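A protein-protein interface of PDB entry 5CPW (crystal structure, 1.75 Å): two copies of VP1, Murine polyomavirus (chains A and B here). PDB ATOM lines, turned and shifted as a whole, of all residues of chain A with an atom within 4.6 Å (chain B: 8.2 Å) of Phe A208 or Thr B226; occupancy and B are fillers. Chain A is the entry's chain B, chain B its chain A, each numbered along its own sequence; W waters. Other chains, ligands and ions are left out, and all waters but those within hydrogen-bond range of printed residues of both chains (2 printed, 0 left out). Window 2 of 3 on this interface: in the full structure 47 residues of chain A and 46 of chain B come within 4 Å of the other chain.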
ATOM      1  N   HIS A 131     -23.561  -3.741   2.197  1.00  0.00           N
ATOM      2  CA  HIS A 131     -24.030  -4.062   0.848  1.00  0.00           C
ATOM      3  C   HIS A 131     -22.814  -4.351   0.011  1.00  0.00           C
ATOM      4  O   HIS A 131     -21.989  -3.470  -0.177  1.00  0.00           O
ATOM      5  CB  HIS A 131     -24.800  -2.887   0.259  1.00  0.00           C
ATOM      6  CG  HIS A 131     -26.087  -2.609   0.969  1.00  0.00           C
ATOM      7  ND1 HIS A 131     -27.197  -3.408   0.812  1.00  0.00           N
ATOM      8  CD2 HIS A 131     -26.428  -1.661   1.873  1.00  0.00           C
ATOM      9  CE1 HIS A 131     -28.180  -2.945   1.564  1.00  0.00           C
ATOM     10  NE2 HIS A 131     -27.736  -1.891   2.225  1.00  0.00           N
ATOM     11  N   VAL A 132     -22.684  -5.595  -0.447  1.00  0.00           N
ATOM     12  CA  VAL A 132     -21.592  -5.974  -1.340  1.00  0.00           C
ATOM     13  C   VAL A 132     -22.174  -6.841  -2.449  1.00  0.00           C
ATOM     14  O   VAL A 132     -23.048  -7.676  -2.200  1.00  0.00           O
ATOM     15  CB  VAL A 132     -20.485  -6.796  -0.629  1.00  0.00           C
ATOM     16  CG1 VAL A 132     -19.235  -6.849  -1.500  1.00  0.00           C
ATOM     17  CG2 VAL A 132     -20.151  -6.225   0.741  1.00  0.00           C
ATOM     18  N   PHE A 133     -21.715  -6.628  -3.673  1.00  0.00           N
ATOM     19  CA  PHE A 133     -21.992  -7.595  -4.736  1.00  0.00           C
ATOM     20  C   PHE A 133     -20.740  -7.829  -5.576  1.00  0.00           C
ATOM     21  O   PHE A 133     -19.835  -6.991  -5.616  1.00  0.00           O
ATOM     22  CB  PHE A 133     -23.209  -7.197  -5.605  1.00  0.00           C
ATOM     23  CG  PHE A 133     -22.955  -6.044  -6.547  1.00  0.00           C
ATOM     24  CD1 PHE A 133     -23.066  -4.723  -6.105  1.00  0.00           C
ATOM     25  CD2 PHE A 133     -22.613  -6.280  -7.877  1.00  0.00           C
ATOM     26  CE1 PHE A 133     -22.836  -3.662  -6.974  1.00  0.00           C
ATOM     27  CE2 PHE A 133     -22.388  -5.221  -8.748  1.00  0.00           C
ATOM     28  CZ  PHE A 133     -22.500  -3.912  -8.295  1.00  0.00           C
ATOM     29  N   ARG A 206     -15.170  -8.619 -10.367  1.00  0.00           N
ATOM     30  CA  ARG A 206     -15.346  -7.237  -9.910  1.00  0.00           C
ATOM     31  C   ARG A 206     -16.243  -7.237  -8.689  1.00  0.00           C
ATOM     32  O   ARG A 206     -17.305  -7.864  -8.701  1.00  0.00           O
ATOM     33  CB  ARG A 206     -15.956  -6.348 -11.001  1.00  0.00           C
ATOM     34  CG  ARG A 206     -15.378  -6.518 -12.402  1.00  0.00           C
ATOM     35  CD  ARG A 206     -13.892  -6.163 -12.483  1.00  0.00           C
ATOM     36  NE  ARG A 206     -13.473  -6.331 -13.865  1.00  0.00           N
ATOM     37  CZ  ARG A 206     -12.626  -7.246 -14.315  1.00  0.00           C
ATOM     38  NH1 ARG A 206     -12.000  -8.083 -13.489  1.00  0.00           N
ATOM     39  NH2 ARG A 206     -12.381  -7.292 -15.607  1.00  0.00           N
ATOM     40  N   TYR A 207     -15.821  -6.558  -7.624  1.00  0.00           N
ATOM     41  CA  TYR A 207     -16.677  -6.432  -6.448  1.00  0.00           C
ATOM     42  C   TYR A 207     -16.814  -4.975  -6.003  1.00  0.00           C
ATOM     43  O   TYR A 207     -15.941  -4.147  -6.283  1.00  0.00           O
ATOM     44  CB  TYR A 207     -16.195  -7.326  -5.293  1.00  0.00           C
ATOM     45  CG  TYR A 207     -14.816  -6.986  -4.757  1.00  0.00           C
ATOM     46  CD1 TYR A 207     -14.634  -5.961  -3.826  1.00  0.00           C
ATOM     47  CD2 TYR A 207     -13.699  -7.708  -5.157  1.00  0.00           C
ATOM     48  CE1 TYR A 207     -13.370  -5.656  -3.334  1.00  0.00           C
ATOM     49  CE2 TYR A 207     -12.437  -7.409  -4.669  1.00  0.00           C
ATOM     50  CZ  TYR A 207     -12.282  -6.381  -3.757  1.00  0.00           C
ATOM     51  OH  TYR A 207     -11.030  -6.098  -3.273  1.00  0.00           O
ATOM     52  N   PHE A 208     -17.919  -4.688  -5.308  1.00  0.00           N
ATOM     53  CA  PHE A 208     -18.312  -3.327  -4.940  1.00  0.00           C
ATOM     54  C   PHE A 208     -19.001  -3.429  -3.597  1.00  0.00           C
ATOM     55  O   PHE A 208     -20.040  -4.086  -3.478  1.00  0.00           O
ATOM     56  CB  PHE A 208     -19.304  -2.743  -5.959  1.00  0.00           C
ATOM     57  CG  PHE A 208     -18.887  -2.911  -7.401  1.00  0.00           C
ATOM     58  CD1 PHE A 208     -19.146  -4.097  -8.085  1.00  0.00           C
ATOM     59  CD2 PHE A 208     -18.248  -1.880  -8.072  1.00  0.00           C
ATOM     60  CE1 PHE A 208     -18.759  -4.251  -9.414  1.00  0.00           C
ATOM     61  CE2 PHE A 208     -17.869  -2.016  -9.400  1.00  0.00           C
ATOM     62  CZ  PHE A 208     -18.120  -3.203 -10.072  1.00  0.00           C
ATOM     63  N   GLY A 209     -18.426  -2.793  -2.581  1.00  0.00           N
ATOM     64  CA  GLY A 209     -18.972  -2.909  -1.232  1.00  0.00           C
ATOM     65  C   GLY A 209     -19.091  -1.591  -0.503  1.00  0.00           C
ATOM     66  O   GLY A 209     -18.338  -0.633  -0.763  1.00  0.00           O
ATOM     67  N   ASN A 210     -20.057  -1.529   0.408  1.00  0.00           N
ATOM     68  CA  ASN A 210     -20.125  -0.404   1.333  1.00  0.00           C
ATOM     69  C   ASN A 210     -20.679  -0.806   2.693  1.00  0.00           C
ATOM     70  O   ASN A 210     -21.513  -1.711   2.796  1.00  0.00           O
ATOM     71  CB  ASN A 210     -20.882   0.789   0.740  1.00  0.00           C
ATOM     72  CG  ASN A 210     -22.306   0.456   0.370  1.00  0.00           C
ATOM     73  OD1 ASN A 210     -23.146   0.234   1.234  1.00  0.00           O
ATOM     74  ND2 ASN A 210     -22.592   0.439  -0.925  1.00  0.00           N
ATOM     75  N   THR A 229     -23.922  -1.306 -14.362  1.00  0.00           N
ATOM     76  CA  THR A 229     -22.547  -1.397 -13.864  1.00  0.00           C
ATOM     77  C   THR A 229     -21.638  -2.048 -14.915  1.00  0.00           C
ATOM     78  O   THR A 229     -21.804  -3.224 -15.236  1.00  0.00           O
ATOM     79  CB  THR A 229     -22.494  -2.202 -12.553  1.00  0.00           C
ATOM     80  OG1 THR A 229     -23.371  -1.608 -11.588  1.00  0.00           O
ATOM     81  CG2 THR A 229     -21.076  -2.249 -11.982  1.00  0.00           C
ATOM     82  N   LEU A 231     -18.432  -3.889 -16.300  1.00  0.00           N
ATOM     83  CA  LEU A 231     -17.513  -4.846 -15.654  1.00  0.00           C
ATOM     84  C   LEU A 231     -16.159  -4.957 -16.356  1.00  0.00           C
ATOM     85  O   LEU A 231     -15.282  -5.710 -15.921  1.00  0.00           O
ATOM     86  CB  LEU A 231     -18.173  -6.231 -15.526  1.00  0.00           C
ATOM     87  CG  LEU A 231     -19.464  -6.302 -14.700  1.00  0.00           C
ATOM     88  CD1 LEU A 231     -20.134  -7.658 -14.876  1.00  0.00           C
ATOM     89  CD2 LEU A 231     -19.201  -6.029 -13.222  1.00  0.00           C
ATOM     90  N   LYS B  94      -4.107   1.310  -6.805  1.00  0.00           N
ATOM     91  CA  LYS B  94      -5.386   0.822  -6.326  1.00  0.00           C
ATOM     92  C   LYS B  94      -5.191   0.546  -4.846  1.00  0.00           C
ATOM     93  O   LYS B  94      -4.286  -0.204  -4.459  1.00  0.00           O
ATOM     94  CB  LYS B  94      -5.809  -0.433  -7.091  1.00  0.00           C
ATOM     95  CG  LYS B  94      -6.005  -0.162  -8.576  1.00  0.00           C
ATOM     96  CD  LYS B  94      -6.296  -1.428  -9.365  1.00  0.00           C
ATOM     97  CE  LYS B  94      -7.790  -1.662  -9.477  1.00  0.00           C
ATOM     98  NZ  LYS B  94      -8.100  -2.725 -10.473  1.00  0.00           N
ATOM     99  N   THR B  95      -5.998   1.197  -4.015  1.00  0.00           N
ATOM    100  CA  THR B  95      -5.872   1.023  -2.572  1.00  0.00           C
ATOM    101  C   THR B  95      -7.242   0.725  -1.969  1.00  0.00           C
ATOM    102  O   THR B  95      -8.257   1.237  -2.446  1.00  0.00           O
ATOM    103  CB  THR B  95      -5.165   2.225  -1.895  1.00  0.00           C
ATOM    104  OG1 THR B  95      -4.976   1.949  -0.506  1.00  0.00           O
ATOM    105  CG2 THR B  95      -5.973   3.535  -2.038  1.00  0.00           C
ATOM    106  N   GLU B  96      -7.254  -0.120  -0.942  1.00  0.00           N
ATOM    107  CA  GLU B  96      -8.491  -0.597  -0.327  1.00  0.00           C
ATOM    108  C   GLU B  96      -8.269  -0.818   1.165  1.00  0.00           C
ATOM    109  O   GLU B  96      -7.240  -1.363   1.561  1.00  0.00           O
ATOM    110  CB  GLU B  96      -8.903  -1.918  -0.996  1.00  0.00           C
ATOM    111  CG  GLU B  96     -10.211  -2.504  -0.482  1.00  0.00           C
ATOM    112  CD  GLU B  96     -10.775  -3.569  -1.412  1.00  0.00           C
ATOM    113  OE1 GLU B  96     -10.415  -3.593  -2.605  1.00  0.00           O
ATOM    114  OE2 GLU B  96     -11.584  -4.381  -0.942  1.00  0.00           O
ATOM    115  N   GLN B 222     -16.249   2.482   2.002  1.00  0.00           N
ATOM    116  CA  GLN B 222     -16.524   1.827   0.727  1.00  0.00           C
ATOM    117  C   GLN B 222     -15.296   1.032   0.323  1.00  0.00           C
ATOM    118  O   GLN B 222     -14.171   1.353   0.730  1.00  0.00           O
ATOM    119  CB  GLN B 222     -16.885   2.839  -0.365  1.00  0.00           C
ATOM    120  CG  GLN B 222     -18.174   3.607  -0.109  1.00  0.00           C
ATOM    121  CD  GLN B 222     -17.937   4.942   0.571  1.00  0.00           C
ATOM    122  OE1 GLN B 222     -17.149   5.761   0.095  1.00  0.00           O
ATOM    123  NE2 GLN B 222     -18.631   5.175   1.680  1.00  0.00           N
ATOM    124  N   PHE B 223     -15.515  -0.021  -0.453  1.00  0.00           N
ATOM    125  CA  PHE B 223     -14.411  -0.850  -0.924  1.00  0.00           C
ATOM    126  C   PHE B 223     -14.771  -1.492  -2.245  1.00  0.00           C
ATOM    127  O   PHE B 223     -15.891  -1.975  -2.436  1.00  0.00           O
ATOM    128  CB  PHE B 223     -13.966  -1.888   0.132  1.00  0.00           C
ATOM    129  CG  PHE B 223     -15.081  -2.749   0.678  1.00  0.00           C
ATOM    130  CD1 PHE B 223     -15.909  -2.281   1.690  1.00  0.00           C
ATOM    131  CD2 PHE B 223     -15.276  -4.048   0.200  1.00  0.00           C
ATOM    132  CE1 PHE B 223     -16.927  -3.069   2.203  1.00  0.00           C
ATOM    133  CE2 PHE B 223     -16.295  -4.844   0.717  1.00  0.00           C
ATOM    134  CZ  PHE B 223     -17.119  -4.351   1.723  1.00  0.00           C
ATOM    135  N   THR B 224     -13.825  -1.443  -3.178  1.00  0.00           N
ATOM    136  CA  THR B 224     -14.012  -2.026  -4.495  1.00  0.00           C
ATOM    137  C   THR B 224     -12.637  -2.272  -5.098  1.00  0.00           C
ATOM    138  O   THR B 224     -11.674  -1.589  -4.736  1.00  0.00           O
ATOM    139  CB  THR B 224     -14.855  -1.118  -5.428  1.00  0.00           C
ATOM    140  OG1 THR B 224     -15.004  -1.746  -6.704  1.00  0.00           O
ATOM    141  CG2 THR B 224     -14.220   0.278  -5.619  1.00  0.00           C
ATOM    142  N   ASN B 225     -12.545  -3.251  -5.993  1.00  0.00           N
ATOM    143  CA  ASN B 225     -11.297  -3.492  -6.722  1.00  0.00           C
ATOM    144  C   ASN B 225     -11.274  -2.808  -8.086  1.00  0.00           C
ATOM    145  O   ASN B 225     -10.430  -3.122  -8.936  1.00  0.00           O
ATOM    146  CB  ASN B 225     -10.981  -5.000  -6.825  1.00  0.00           C
ATOM    147  CG  ASN B 225     -12.004  -5.780  -7.639  1.00  0.00           C
ATOM    148  OD1 ASN B 225     -13.137  -5.332  -7.856  1.00  0.00           O
ATOM    149  ND2 ASN B 225     -11.599  -6.965  -8.105  1.00  0.00           N
ATOM    150  N   THR B 226     -12.197  -1.865  -8.296  1.00  0.00           N
ATOM    151  CA  THR B 226     -12.390  -1.270  -9.631  1.00  0.00           C
ATOM    152  C   THR B 226     -11.969   0.200  -9.704  1.00  0.00           C
ATOM    153  O   THR B 226     -12.123   0.825 -10.757  1.00  0.00           O
ATOM    154  CB  THR B 226     -13.864  -1.330 -10.090  1.00  0.00           C
ATOM    155  OG1 THR B 226     -14.671  -0.519  -9.219  1.00  0.00           O
ATOM    156  CG2 THR B 226     -14.387  -2.774 -10.108  1.00  0.00           C
ATOM    157  N   LEU B 227     -11.463   0.732  -8.593  1.00  0.00           N
ATOM    158  CA  LEU B 227     -11.106   2.147  -8.496  1.00  0.00           C
ATOM    159  C   LEU B 227      -9.594   2.369  -8.525  1.00  0.00           C
ATOM    160  O   LEU B 227      -8.858   1.832  -7.701  1.00  0.00           O
ATOM    161  CB  LEU B 227     -11.712   2.750  -7.221  1.00  0.00           C
ATOM    162  CG  LEU B 227     -11.479   4.224  -6.867  1.00  0.00           C
ATOM    163  CD1 LEU B 227     -12.125   5.145  -7.895  1.00  0.00           C
ATOM    164  CD2 LEU B 227     -12.008   4.519  -5.468  1.00  0.00           C
ATOM    165  N   THR B 228      -9.147   3.174  -9.478  1.00  0.00           N
ATOM    166  CA  THR B 228      -7.741   3.515  -9.602  1.00  0.00           C
ATOM    167  C   THR B 228      -7.534   4.988  -9.243  1.00  0.00           C
ATOM    168  O   THR B 228      -8.251   5.863  -9.750  1.00  0.00           O
ATOM    169  CB  THR B 228      -7.280   3.244 -11.041  1.00  0.00           C
ATOM    170  OG1 THR B 228      -7.379   1.837 -11.296  1.00  0.00           O
ATOM    171  CG2 THR B 228      -5.843   3.705 -11.265  1.00  0.00           C
ATOM    172  N   THR B 229      -6.552   5.248  -8.381  1.00  0.00           N
ATOM    173  CA  THR B 229      -6.140   6.609  -8.041  1.00  0.00           C
ATOM    174  C   THR B 229      -4.919   6.984  -8.889  1.00  0.00           C
ATOM    175  O   THR B 229      -3.869   6.353  -8.765  1.00  0.00           O
ATOM    176  CB  THR B 229      -5.766   6.705  -6.542  1.00  0.00           C
ATOM    177  OG1 THR B 229      -6.869   6.274  -5.728  1.00  0.00           O
ATOM    178  CG2 THR B 229      -5.387   8.126  -6.159  1.00  0.00           C
HETATM  179  O   HOH W   1     -10.349  -7.555 -11.169  1.00  0.00           O
HETATM  180  O   HOH W   2     -17.885   0.459  -3.544  1.00  0.00           O
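OE1 of Glu B96 lies within hydrogen-bond range of OH of Tyr A207, at 2.7 Å.
The backbone NH (N) of Gly A209 is in hydrogen-bond range of the backbone carbonyl oxygen (O) of Phe B223, 2.7 Å away.
O of Tyr A207 lies within hydrogen-bond range of OG1 of Thr B224 (2.6 Å).
OD1 of Asn B225 is in hydrogen-bond range of N of Tyr A207 (3.0 Å).
The side-chain amino group of Lys B94 is in hydrogen-bond range of the backbone carbonyl oxygen of Asn B225, at 2.8 Å.
The side-chain hydroxyl of Thr B226 is in hydrogen-bond range of the side-chain hydroxyl of Thr B224, 2.8 Å away.
O of His A131 sits at hydrogen-bond distance from N of Asn A210.
O of Phe A133 is in hydrogen-bond range of N of Phe A208 (3.0 Å).
The guanidinium group (NE) of Arg A206 sits at hydrogen-bond distance from the backbone carbonyl oxygen (O) of Leu A231, 2.8 Å away.
CZ of Phe B223 touches CG2 of Val A132, 3.7 Å away.
Arg A206 touches Asn B225 (CA to OD1, 3.6 Å).
C of Phe A208 touches O of Phe B223, 3.6 Å away.
Phe A208 touches Thr B224 (CD2 to OG1, 3.5 Å).
Phe A208 touches Thr B226.
Gly A209 touches Gln B222 (O to CA, 3.4 Å).
CB of Asn A210 touches CG of Gln B222, 3.999 Å away.
N of Asn A210 touches CE1 of Phe B223, 3.9 Å away.
His A131 touches none of the printed residues of chain B.
Of the printed residues of chain B, Tyr A207 touches Glu B96, Thr B224 and Asn B225.
Of chain B, only Phe B223, Thr B224 and Thr B226 come within 4 Å of Phe A208.
Printed residues of chain B within 4 Å of Gly A209: Gln B222 (3.4 Å) and Phe B223 (2.7 Å).
Of the printed residues of chain A, Gln B222 touches Gly A209 and Asn A210.
Of the printed residues of chain A, Thr B226 touches Phe A208.
The nearest residue of chain B that does not touch Phe A208 is Asn B225 (5.5 Å).
The nearest printed residue of chain A that does not touch Thr B226 is Arg A206 (4.004 Å).
Of the 11 printed residues of chain B, 6 touch a printed residue of chain A.
Printed residues of chain B that touch a printed residue of chain A: Glu B96, Gln B222, Phe B223, Thr B224, Asn B225 and Thr B226.
Hydrophobic or aromatic side chains of chain B within 4 Å of the printed part of chain A: Phe B223.
Along chain B the printed residues that touch a printed residue of chain A span positions 96 to 226.
Of the 10 printed residues of chain A, 6 touch a printed residue of chain B.
Printed residues of chain A that touch a printed residue of chain B: Val A132, Arg A206, Tyr A207, Phe A208, Gly A209 and Asn A210.
Hydrophobic or aromatic side chains of chain A within 4 Å of the printed part of chain B: Val A132, Tyr A207 and Phe A208.
Along chain A the printed residues that touch a printed residue of chain B span positions 132 to 210.
Position printed for both chains: 229.
Of the 12 pairs that touch across the chains among the printed residues, none has its exchanged pair printed and touching as well.
Water W1 bridges the guanidinium group (NH1) of Arg A206 (2.9 Å) and the side-chain amide nitrogen (ND2) of Asn B225 (3.4 Å).
Water W2 lies within hydrogen-bond range of O of Gly A209 (3.0 Å) and O of Phe B223 (3.3 Å).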
